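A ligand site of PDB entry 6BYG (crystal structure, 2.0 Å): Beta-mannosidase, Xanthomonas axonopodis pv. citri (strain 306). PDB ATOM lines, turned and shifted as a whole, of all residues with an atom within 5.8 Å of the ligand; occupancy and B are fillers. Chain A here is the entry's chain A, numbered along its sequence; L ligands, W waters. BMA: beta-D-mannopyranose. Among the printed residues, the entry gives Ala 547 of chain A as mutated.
ND1 of His 522 sits at hydrogen-bond distance from OE2 of Glu 449 (2.6 Å).
ND2 of Asn 448 is in hydrogen-bond range of OE1 of Glu 449 (3.1 Å).
NE1 of Trp 188 sits close to OD1 of Asp 187 (3.4 Å).
OD2 of Asp 187 sits at hydrogen-bond distance from OH of Tyr 160.
The side-chain amide nitrogen of Asn 448 lies close to the indole nitrogen of Trp 382.
The side-chain amide oxygen (OE1) of Gln 640 lies within hydrogen-bond range of the indole nitrogen (NE1) of Trp 639.
The backbone carbonyl oxygen (O) of Trp 650 lies within hydrogen-bond range of the backbone NH (N) of Gln 640 (3.1 Å).
OD1 of Asn 448 is in hydrogen-bond range of NH2 of Arg 380 (2.9 Å).
Water W2 lies within hydrogen-bond range of O3 of the ligand and OH of Tyr 160.
Water W3 lies within hydrogen-bond range of the side-chain amide oxygen (OD1) of Asn 448 (2.7 Å), an oxygen (O1) of the ligand (2.8 Å), the guanidinium group (NH1) of Arg 380 (3.0 Å) and a ring nitrogen (ND1) of His 522 (3.4 Å).
An oxygen (O2) of the ligand sits at hydrogen-bond distance from the side-chain carboxylate of Glu 449, at 2.4 Å.
O4 of the ligand is in hydrogen-bond range of OD1 of Asp 187 (2.6 Å).
NE1 of Trp 186 lies within hydrogen-bond range of O3 of the ligand (2.8 Å).
The indole nitrogen (NE1) of Trp 188 lies within hydrogen-bond range of an oxygen (O4) of the ligand (2.9 Å).
NE1 of Trp 524 lies within hydrogen-bond range of O1 of the ligand, at 3.0 Å.
The indole nitrogen of Trp 382 lies within hydrogen-bond range of an oxygen (O3) of the ligand (3.2 Å).
Asn 448 touches the ligand.
His 522 touches the ligand (ND1 to O1, 3.7 Å).
CB of Ala 547 touches O1 of the ligand, at 3.9 Å.
Trp 639 touches the ligand.
Trp 650 touches the ligand.
Hydrophobic or aromatic side chains within 4 Å of the ligand: Trp 186, Trp 188, Trp 382, Trp 524, Ala 547, Trp 639 and Trp 650.
Within 4 Å of the ligand: Trp 186, Asp 187, Trp 188, Trp 382, Asn 448, Glu 449, His 522, Trp 524, Ala 547, Trp 639 and Trp 650.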
ATOM      1  N   TYR A 160     -29.748 -11.733   6.852  1.00  0.00           N
ATOM      2  CA  TYR A 160     -29.206 -11.259   8.113  1.00  0.00           C
ATOM      3  C   TYR A 160     -29.628  -9.841   8.342  1.00  0.00           C
ATOM      4  O   TYR A 160     -29.684  -9.038   7.413  1.00  0.00           O
ATOM      5  CB  TYR A 160     -27.678 -11.410   8.147  1.00  0.00           C
ATOM      6  CG  TYR A 160     -27.261 -12.867   8.181  1.00  0.00           C
ATOM      7  CD1 TYR A 160     -27.216 -13.626   7.004  1.00  0.00           C
ATOM      8  CD2 TYR A 160     -26.970 -13.504   9.382  1.00  0.00           C
ATOM      9  CE1 TYR A 160     -26.876 -14.968   7.023  1.00  0.00           C
ATOM     10  CE2 TYR A 160     -26.614 -14.860   9.401  1.00  0.00           C
ATOM     11  CZ  TYR A 160     -26.571 -15.577   8.229  1.00  0.00           C
ATOM     12  OH  TYR A 160     -26.231 -16.904   8.247  1.00  0.00           O
ATOM     13  N   TRP A 186     -23.213 -11.567   5.686  1.00  0.00           N
ATOM     14  CA  TRP A 186     -23.449 -12.975   5.956  1.00  0.00           C
ATOM     15  C   TRP A 186     -22.645 -13.338   7.198  1.00  0.00           C
ATOM     16  O   TRP A 186     -22.003 -12.457   7.772  1.00  0.00           O
ATOM     17  CB  TRP A 186     -23.038 -13.857   4.775  1.00  0.00           C
ATOM     18  CG  TRP A 186     -23.930 -15.081   4.596  1.00  0.00           C
ATOM     19  CD1 TRP A 186     -23.646 -16.367   4.953  1.00  0.00           C
ATOM     20  CD2 TRP A 186     -25.240 -15.099   3.995  1.00  0.00           C
ATOM     21  NE1 TRP A 186     -24.706 -17.186   4.631  1.00  0.00           N
ATOM     22  CE2 TRP A 186     -25.692 -16.442   4.036  1.00  0.00           C
ATOM     23  CE3 TRP A 186     -26.069 -14.124   3.424  1.00  0.00           C
ATOM     24  CZ2 TRP A 186     -26.938 -16.823   3.531  1.00  0.00           C
ATOM     25  CZ3 TRP A 186     -27.309 -14.498   2.923  1.00  0.00           C
ATOM     26  CH2 TRP A 186     -27.743 -15.848   2.976  1.00  0.00           C
ATOM     27  N   ASP A 187     -22.687 -14.605   7.621  1.00  0.00           N
ATOM     28  CA  ASP A 187     -22.066 -14.958   8.889  1.00  0.00           C
ATOM     29  C   ASP A 187     -20.558 -15.250   8.772  1.00  0.00           C
ATOM     30  O   ASP A 187     -19.921 -15.587   9.775  1.00  0.00           O
ATOM     31  CB  ASP A 187     -22.819 -16.127   9.587  1.00  0.00           C
ATOM     32  CG  ASP A 187     -22.791 -17.466   8.814  1.00  0.00           C
ATOM     33  OD1 ASP A 187     -22.222 -17.608   7.705  1.00  0.00           O
ATOM     34  OD2 ASP A 187     -23.381 -18.429   9.354  1.00  0.00           O
ATOM     35  N   TRP A 188     -19.995 -15.044   7.581  1.00  0.00           N
ATOM     36  CA  TRP A 188     -18.522 -15.016   7.380  1.00  0.00           C
ATOM     37  C   TRP A 188     -18.047 -13.821   6.538  1.00  0.00           C
ATOM     38  O   TRP A 188     -16.898 -13.788   6.107  1.00  0.00           O
ATOM     39  CB  TRP A 188     -18.030 -16.321   6.718  1.00  0.00           C
ATOM     40  CG  TRP A 188     -19.013 -16.879   5.735  1.00  0.00           C
ATOM     41  CD1 TRP A 188     -19.742 -18.046   5.865  1.00  0.00           C
ATOM     42  CD2 TRP A 188     -19.442 -16.283   4.488  1.00  0.00           C
ATOM     43  NE1 TRP A 188     -20.573 -18.214   4.776  1.00  0.00           N
ATOM     44  CE2 TRP A 188     -20.412 -17.143   3.918  1.00  0.00           C
ATOM     45  CE3 TRP A 188     -19.099 -15.104   3.790  1.00  0.00           C
ATOM     46  CZ2 TRP A 188     -21.028 -16.885   2.700  1.00  0.00           C
ATOM     47  CZ3 TRP A 188     -19.732 -14.831   2.571  1.00  0.00           C
ATOM     48  CH2 TRP A 188     -20.684 -15.724   2.040  1.00  0.00           C
ATOM     49  N   ARG A 380     -19.279 -27.359  -4.345  1.00  0.00           N
ATOM     50  CA  ARG A 380     -20.634 -26.855  -4.478  1.00  0.00           C
ATOM     51  C   ARG A 380     -20.605 -25.345  -4.439  1.00  0.00           C
ATOM     52  O   ARG A 380     -20.151 -24.730  -3.452  1.00  0.00           O
ATOM     53  CB  ARG A 380     -21.547 -27.389  -3.374  1.00  0.00           C
ATOM     54  CG  ARG A 380     -22.868 -26.581  -3.213  1.00  0.00           C
ATOM     55  CD  ARG A 380     -23.832 -27.314  -2.284  1.00  0.00           C
ATOM     56  NE  ARG A 380     -25.022 -26.498  -2.052  1.00  0.00           N
ATOM     57  CZ  ARG A 380     -25.375 -26.023  -0.858  1.00  0.00           C
ATOM     58  NH1 ARG A 380     -24.639 -26.313   0.225  1.00  0.00           N
ATOM     59  NH2 ARG A 380     -26.457 -25.244  -0.756  1.00  0.00           N
ATOM     60  N   TRP A 382     -22.409 -22.385  -3.747  1.00  0.00           N
ATOM     61  CA  TRP A 382     -23.534 -22.141  -2.847  1.00  0.00           C
ATOM     62  C   TRP A 382     -24.378 -20.921  -3.242  1.00  0.00           C
ATOM     63  O   TRP A 382     -23.814 -19.853  -3.585  1.00  0.00           O
ATOM     64  CB  TRP A 382     -22.955 -22.031  -1.435  1.00  0.00           C
ATOM     65  CG  TRP A 382     -23.681 -21.206  -0.388  1.00  0.00           C
ATOM     66  CD1 TRP A 382     -24.558 -21.666   0.540  1.00  0.00           C
ATOM     67  CD2 TRP A 382     -23.506 -19.809  -0.124  1.00  0.00           C
ATOM     68  NE1 TRP A 382     -24.967 -20.633   1.370  1.00  0.00           N
ATOM     69  CE2 TRP A 382     -24.333 -19.480   0.979  1.00  0.00           C
ATOM     70  CE3 TRP A 382     -22.732 -18.802  -0.718  1.00  0.00           C
ATOM     71  CZ2 TRP A 382     -24.422 -18.184   1.492  1.00  0.00           C
ATOM     72  CZ3 TRP A 382     -22.816 -17.513  -0.200  1.00  0.00           C
ATOM     73  CH2 TRP A 382     -23.668 -17.212   0.890  1.00  0.00           C
ATOM     74  N   GLY A 410     -30.296 -18.086  -1.499  1.00  0.00           N
ATOM     75  CA  GLY A 410     -29.473 -18.424  -0.355  1.00  0.00           C
ATOM     76  C   GLY A 410     -30.189 -18.893   0.914  1.00  0.00           C
ATOM     77  O   GLY A 410     -29.536 -19.239   1.904  1.00  0.00           O
ATOM     78  N   ASN A 448     -30.067 -22.823  -1.654  1.00  0.00           N
ATOM     79  CA  ASN A 448     -29.546 -23.220  -0.373  1.00  0.00           C
ATOM     80  C   ASN A 448     -30.620 -23.094   0.729  1.00  0.00           C
ATOM     81  O   ASN A 448     -31.096 -22.006   0.987  1.00  0.00           O
ATOM     82  CB  ASN A 448     -28.332 -22.355  -0.017  1.00  0.00           C
ATOM     83  CG  ASN A 448     -27.775 -22.668   1.348  1.00  0.00           C
ATOM     84  OD1 ASN A 448     -27.193 -23.745   1.560  1.00  0.00           O
ATOM     85  ND2 ASN A 448     -27.975 -21.753   2.289  1.00  0.00           N
ATOM     86  N   GLU A 449     -31.000 -24.224   1.326  1.00  0.00           N
ATOM     87  CA  GLU A 449     -31.650 -24.322   2.639  1.00  0.00           C
ATOM     88  C   GLU A 449     -33.039 -23.718   2.794  1.00  0.00           C
ATOM     89  O   GLU A 449     -33.558 -23.641   3.919  1.00  0.00           O
ATOM     90  CB  GLU A 449     -30.719 -23.738   3.729  1.00  0.00           C
ATOM     91  CG  GLU A 449     -29.478 -24.627   3.884  1.00  0.00           C
ATOM     92  CD  GLU A 449     -28.444 -24.066   4.852  1.00  0.00           C
ATOM     93  OE1 GLU A 449     -28.468 -22.839   5.105  1.00  0.00           O
ATOM     94  OE2 GLU A 449     -27.589 -24.880   5.324  1.00  0.00           O
ATOM     95  N   TRP A 457     -36.146 -24.064  10.980  1.00  0.00           N
ATOM     96  CA  TRP A 457     -35.681 -22.852  11.664  1.00  0.00           C
ATOM     97  C   TRP A 457     -36.851 -22.134  12.372  1.00  0.00           C
ATOM     98  O   TRP A 457     -37.893 -21.865  11.763  1.00  0.00           O
ATOM     99  CB  TRP A 457     -34.992 -21.893  10.676  1.00  0.00           C
ATOM    100  CG  TRP A 457     -33.794 -22.512   9.975  1.00  0.00           C
ATOM    101  CD1 TRP A 457     -33.216 -23.719  10.235  1.00  0.00           C
ATOM    102  CD2 TRP A 457     -33.053 -21.948   8.889  1.00  0.00           C
ATOM    103  NE1 TRP A 457     -32.151 -23.935   9.389  1.00  0.00           N
ATOM    104  CE2 TRP A 457     -32.048 -22.869   8.529  1.00  0.00           C
ATOM    105  CE3 TRP A 457     -33.163 -20.762   8.153  1.00  0.00           C
ATOM    106  CZ2 TRP A 457     -31.134 -22.633   7.497  1.00  0.00           C
ATOM    107  CZ3 TRP A 457     -32.250 -20.527   7.121  1.00  0.00           C
ATOM    108  CH2 TRP A 457     -31.260 -21.456   6.812  1.00  0.00           C
ATOM    109  N   HIS A 522     -27.446 -31.049   5.548  1.00  0.00           N
ATOM    110  CA  HIS A 522     -26.538 -30.057   6.134  1.00  0.00           C
ATOM    111  C   HIS A 522     -26.541 -30.242   7.630  1.00  0.00           C
ATOM    112  O   HIS A 522     -27.582 -30.052   8.293  1.00  0.00           O
ATOM    113  CB  HIS A 522     -26.970 -28.627   5.808  1.00  0.00           C
ATOM    114  CG  HIS A 522     -26.918 -28.290   4.350  1.00  0.00           C
ATOM    115  ND1 HIS A 522     -27.116 -27.027   3.870  1.00  0.00           N
ATOM    116  CD2 HIS A 522     -26.684 -29.091   3.274  1.00  0.00           C
ATOM    117  CE1 HIS A 522     -27.016 -27.042   2.544  1.00  0.00           C
ATOM    118  NE2 HIS A 522     -26.750 -28.284   2.160  1.00  0.00           N
ATOM    119  N   TRP A 524     -25.325 -29.262  11.386  1.00  0.00           N
ATOM    120  CA  TRP A 524     -24.820 -28.124  12.128  1.00  0.00           C
ATOM    121  C   TRP A 524     -25.057 -28.236  13.634  1.00  0.00           C
ATOM    122  O   TRP A 524     -24.953 -27.235  14.340  1.00  0.00           O
ATOM    123  CB  TRP A 524     -25.431 -26.822  11.586  1.00  0.00           C
ATOM    124  CG  TRP A 524     -24.763 -26.413  10.329  1.00  0.00           C
ATOM    125  CD1 TRP A 524     -25.294 -26.376   9.061  1.00  0.00           C
ATOM    126  CD2 TRP A 524     -23.380 -26.004  10.204  1.00  0.00           C
ATOM    127  NE1 TRP A 524     -24.308 -25.962   8.149  1.00  0.00           N
ATOM    128  CE2 TRP A 524     -23.141 -25.731   8.836  1.00  0.00           C
ATOM    129  CE3 TRP A 524     -22.331 -25.839  11.122  1.00  0.00           C
ATOM    130  CZ2 TRP A 524     -21.894 -25.292   8.371  1.00  0.00           C
ATOM    131  CZ3 TRP A 524     -21.091 -25.408  10.653  1.00  0.00           C
ATOM    132  CH2 TRP A 524     -20.881 -25.154   9.292  1.00  0.00           C
ATOM    133  N   TRP A 527     -20.743 -27.410  15.943  1.00  0.00           N
ATOM    134  CA  TRP A 527     -20.532 -25.973  15.750  1.00  0.00           C
ATOM    135  C   TRP A 527     -21.774 -25.198  16.119  1.00  0.00           C
ATOM    136  O   TRP A 527     -21.738 -24.376  17.019  1.00  0.00           O
ATOM    137  CB  TRP A 527     -20.115 -25.569  14.335  1.00  0.00           C
ATOM    138  CG  TRP A 527     -19.919 -24.074  14.363  1.00  0.00           C
ATOM    139  CD1 TRP A 527     -20.795 -23.128  13.921  1.00  0.00           C
ATOM    140  CD2 TRP A 527     -18.826 -23.351  14.968  1.00  0.00           C
ATOM    141  NE1 TRP A 527     -20.292 -21.868  14.160  1.00  0.00           N
ATOM    142  CE2 TRP A 527     -19.095 -21.975  14.823  1.00  0.00           C
ATOM    143  CE3 TRP A 527     -17.632 -23.731  15.591  1.00  0.00           C
ATOM    144  CZ2 TRP A 527     -18.230 -21.000  15.277  1.00  0.00           C
ATOM    145  CZ3 TRP A 527     -16.784 -22.756  16.047  1.00  0.00           C
ATOM    146  CH2 TRP A 527     -17.082 -21.393  15.896  1.00  0.00           C
ATOM    147  N   ALA A 547     -23.113 -30.167   3.569  1.00  0.00           N
ATOM    148  CA  ALA A 547     -22.522 -29.094   4.350  1.00  0.00           C
ATOM    149  C   ALA A 547     -22.383 -29.471   5.839  1.00  0.00           C
ATOM    150  O   ALA A 547     -23.233 -30.181   6.385  1.00  0.00           O
ATOM    151  CB  ALA A 547     -23.351 -27.816   4.207  1.00  0.00           C
ATOM    152  N   PHE A 581     -20.225 -14.685  12.948  1.00  0.00           N
ATOM    153  CA  PHE A 581     -21.179 -15.689  13.416  1.00  0.00           C
ATOM    154  C   PHE A 581     -21.832 -15.206  14.717  1.00  0.00           C
ATOM    155  O   PHE A 581     -21.167 -14.606  15.566  1.00  0.00           O
ATOM    156  CB  PHE A 581     -20.490 -17.064  13.612  1.00  0.00           C
ATOM    157  CG  PHE A 581     -21.420 -18.140  14.164  1.00  0.00           C
ATOM    158  CD1 PHE A 581     -22.341 -18.778  13.337  1.00  0.00           C
ATOM    159  CD2 PHE A 581     -21.391 -18.483  15.508  1.00  0.00           C
ATOM    160  CE1 PHE A 581     -23.209 -19.733  13.842  1.00  0.00           C
ATOM    161  CE2 PHE A 581     -22.248 -19.452  16.022  1.00  0.00           C
ATOM    162  CZ  PHE A 581     -23.163 -20.083  15.198  1.00  0.00           C
ATOM    163  N   TRP A 639     -18.352 -27.325   4.778  1.00  0.00           N
ATOM    164  CA  TRP A 639     -18.490 -25.890   4.780  1.00  0.00           C
ATOM    165  C   TRP A 639     -17.279 -25.298   5.547  1.00  0.00           C
ATOM    166  O   TRP A 639     -17.134 -25.576   6.731  1.00  0.00           O
ATOM    167  CB  TRP A 639     -19.821 -25.489   5.448  1.00  0.00           C
ATOM    168  CG  TRP A 639     -20.006 -24.031   5.299  1.00  0.00           C
ATOM    169  CD1 TRP A 639     -19.499 -23.051   6.109  1.00  0.00           C
ATOM    170  CD2 TRP A 639     -20.627 -23.371   4.196  1.00  0.00           C
ATOM    171  NE1 TRP A 639     -19.816 -21.807   5.592  1.00  0.00           N
ATOM    172  CE2 TRP A 639     -20.507 -21.976   4.414  1.00  0.00           C
ATOM    173  CE3 TRP A 639     -21.317 -23.818   3.075  1.00  0.00           C
ATOM    174  CZ2 TRP A 639     -21.035 -21.035   3.538  1.00  0.00           C
ATOM    175  CZ3 TRP A 639     -21.840 -22.872   2.179  1.00  0.00           C
ATOM    176  CH2 TRP A 639     -21.708 -21.497   2.419  1.00  0.00           C
ATOM    177  N   GLN A 640     -16.389 -24.505   4.920  1.00  0.00           N
ATOM    178  CA  GLN A 640     -16.412 -24.020   3.563  1.00  0.00           C
ATOM    179  C   GLN A 640     -14.985 -24.075   2.998  1.00  0.00           C
ATOM    180  O   GLN A 640     -14.035 -24.261   3.764  1.00  0.00           O
ATOM    181  CB  GLN A 640     -16.909 -22.567   3.538  1.00  0.00           C
ATOM    182  CG  GLN A 640     -15.909 -21.551   4.109  1.00  0.00           C
ATOM    183  CD  GLN A 640     -16.565 -20.374   4.849  1.00  0.00           C
ATOM    184  OE1 GLN A 640     -17.241 -20.565   5.847  1.00  0.00           O
ATOM    185  NE2 GLN A 640     -16.348 -19.155   4.376  1.00  0.00           N
ATOM    186  N   TRP A 650     -15.324 -20.672   8.406  1.00  0.00           N
ATOM    187  CA  TRP A 650     -15.216 -22.120   8.398  1.00  0.00           C
ATOM    188  C   TRP A 650     -14.285 -22.562   7.279  1.00  0.00           C
ATOM    189  O   TRP A 650     -14.197 -23.738   6.977  1.00  0.00           O
ATOM    190  CB  TRP A 650     -16.597 -22.763   8.220  1.00  0.00           C
ATOM    191  CG  TRP A 650     -17.569 -22.437   9.302  1.00  0.00           C
ATOM    192  CD1 TRP A 650     -17.917 -23.239  10.368  1.00  0.00           C
ATOM    193  CD2 TRP A 650     -18.336 -21.235   9.434  1.00  0.00           C
ATOM    194  NE1 TRP A 650     -18.868 -22.601  11.140  1.00  0.00           N
ATOM    195  CE2 TRP A 650     -19.140 -21.370  10.594  1.00  0.00           C
ATOM    196  CE3 TRP A 650     -18.442 -20.052   8.665  1.00  0.00           C
ATOM    197  CZ2 TRP A 650     -20.016 -20.355  11.024  1.00  0.00           C
ATOM    198  CZ3 TRP A 650     -19.319 -19.046   9.084  1.00  0.00           C
ATOM    199  CH2 TRP A 650     -20.083 -19.201  10.273  1.00  0.00           C
HETATM  200  C1  BMA L   1     -24.255 -23.244   5.489  1.00  0.00           C
HETATM  201  C2  BMA L   1     -25.297 -22.203   5.002  1.00  0.00           C
HETATM  202  C3  BMA L   1     -24.590 -20.887   4.863  1.00  0.00           C
HETATM  203  C4  BMA L   1     -23.819 -20.490   6.160  1.00  0.00           C
HETATM  204  C5  BMA L   1     -22.932 -21.672   6.672  1.00  0.00           C
HETATM  205  C6  BMA L   1     -22.227 -21.389   8.012  1.00  0.00           C
HETATM  206  O1  BMA L   1     -24.912 -24.521   5.536  1.00  0.00           O
HETATM  207  O2  BMA L   1     -26.346 -22.046   5.985  1.00  0.00           O
HETATM  208  O3  BMA L   1     -25.477 -19.837   4.461  1.00  0.00           O
HETATM  209  O4  BMA L   1     -22.968 -19.331   5.929  1.00  0.00           O
HETATM  210  O5  BMA L   1     -23.733 -22.860   6.772  1.00  0.00           O
HETATM  211  O6  BMA L   1     -23.204 -21.243   9.066  1.00  0.00           O
HETATM  212  O   HOH W   1     -25.944 -22.426   8.687  1.00  0.00           O
HETATM  213  O   HOH W   2     -27.358 -19.212   6.205  1.00  0.00           O
HETATM  214  O   HOH W   3     -24.983 -24.668   2.737  1.00  0.00           O
HETATM  215  O   HOH W   4     -23.416 -22.538  11.443  1.00  0.00           O
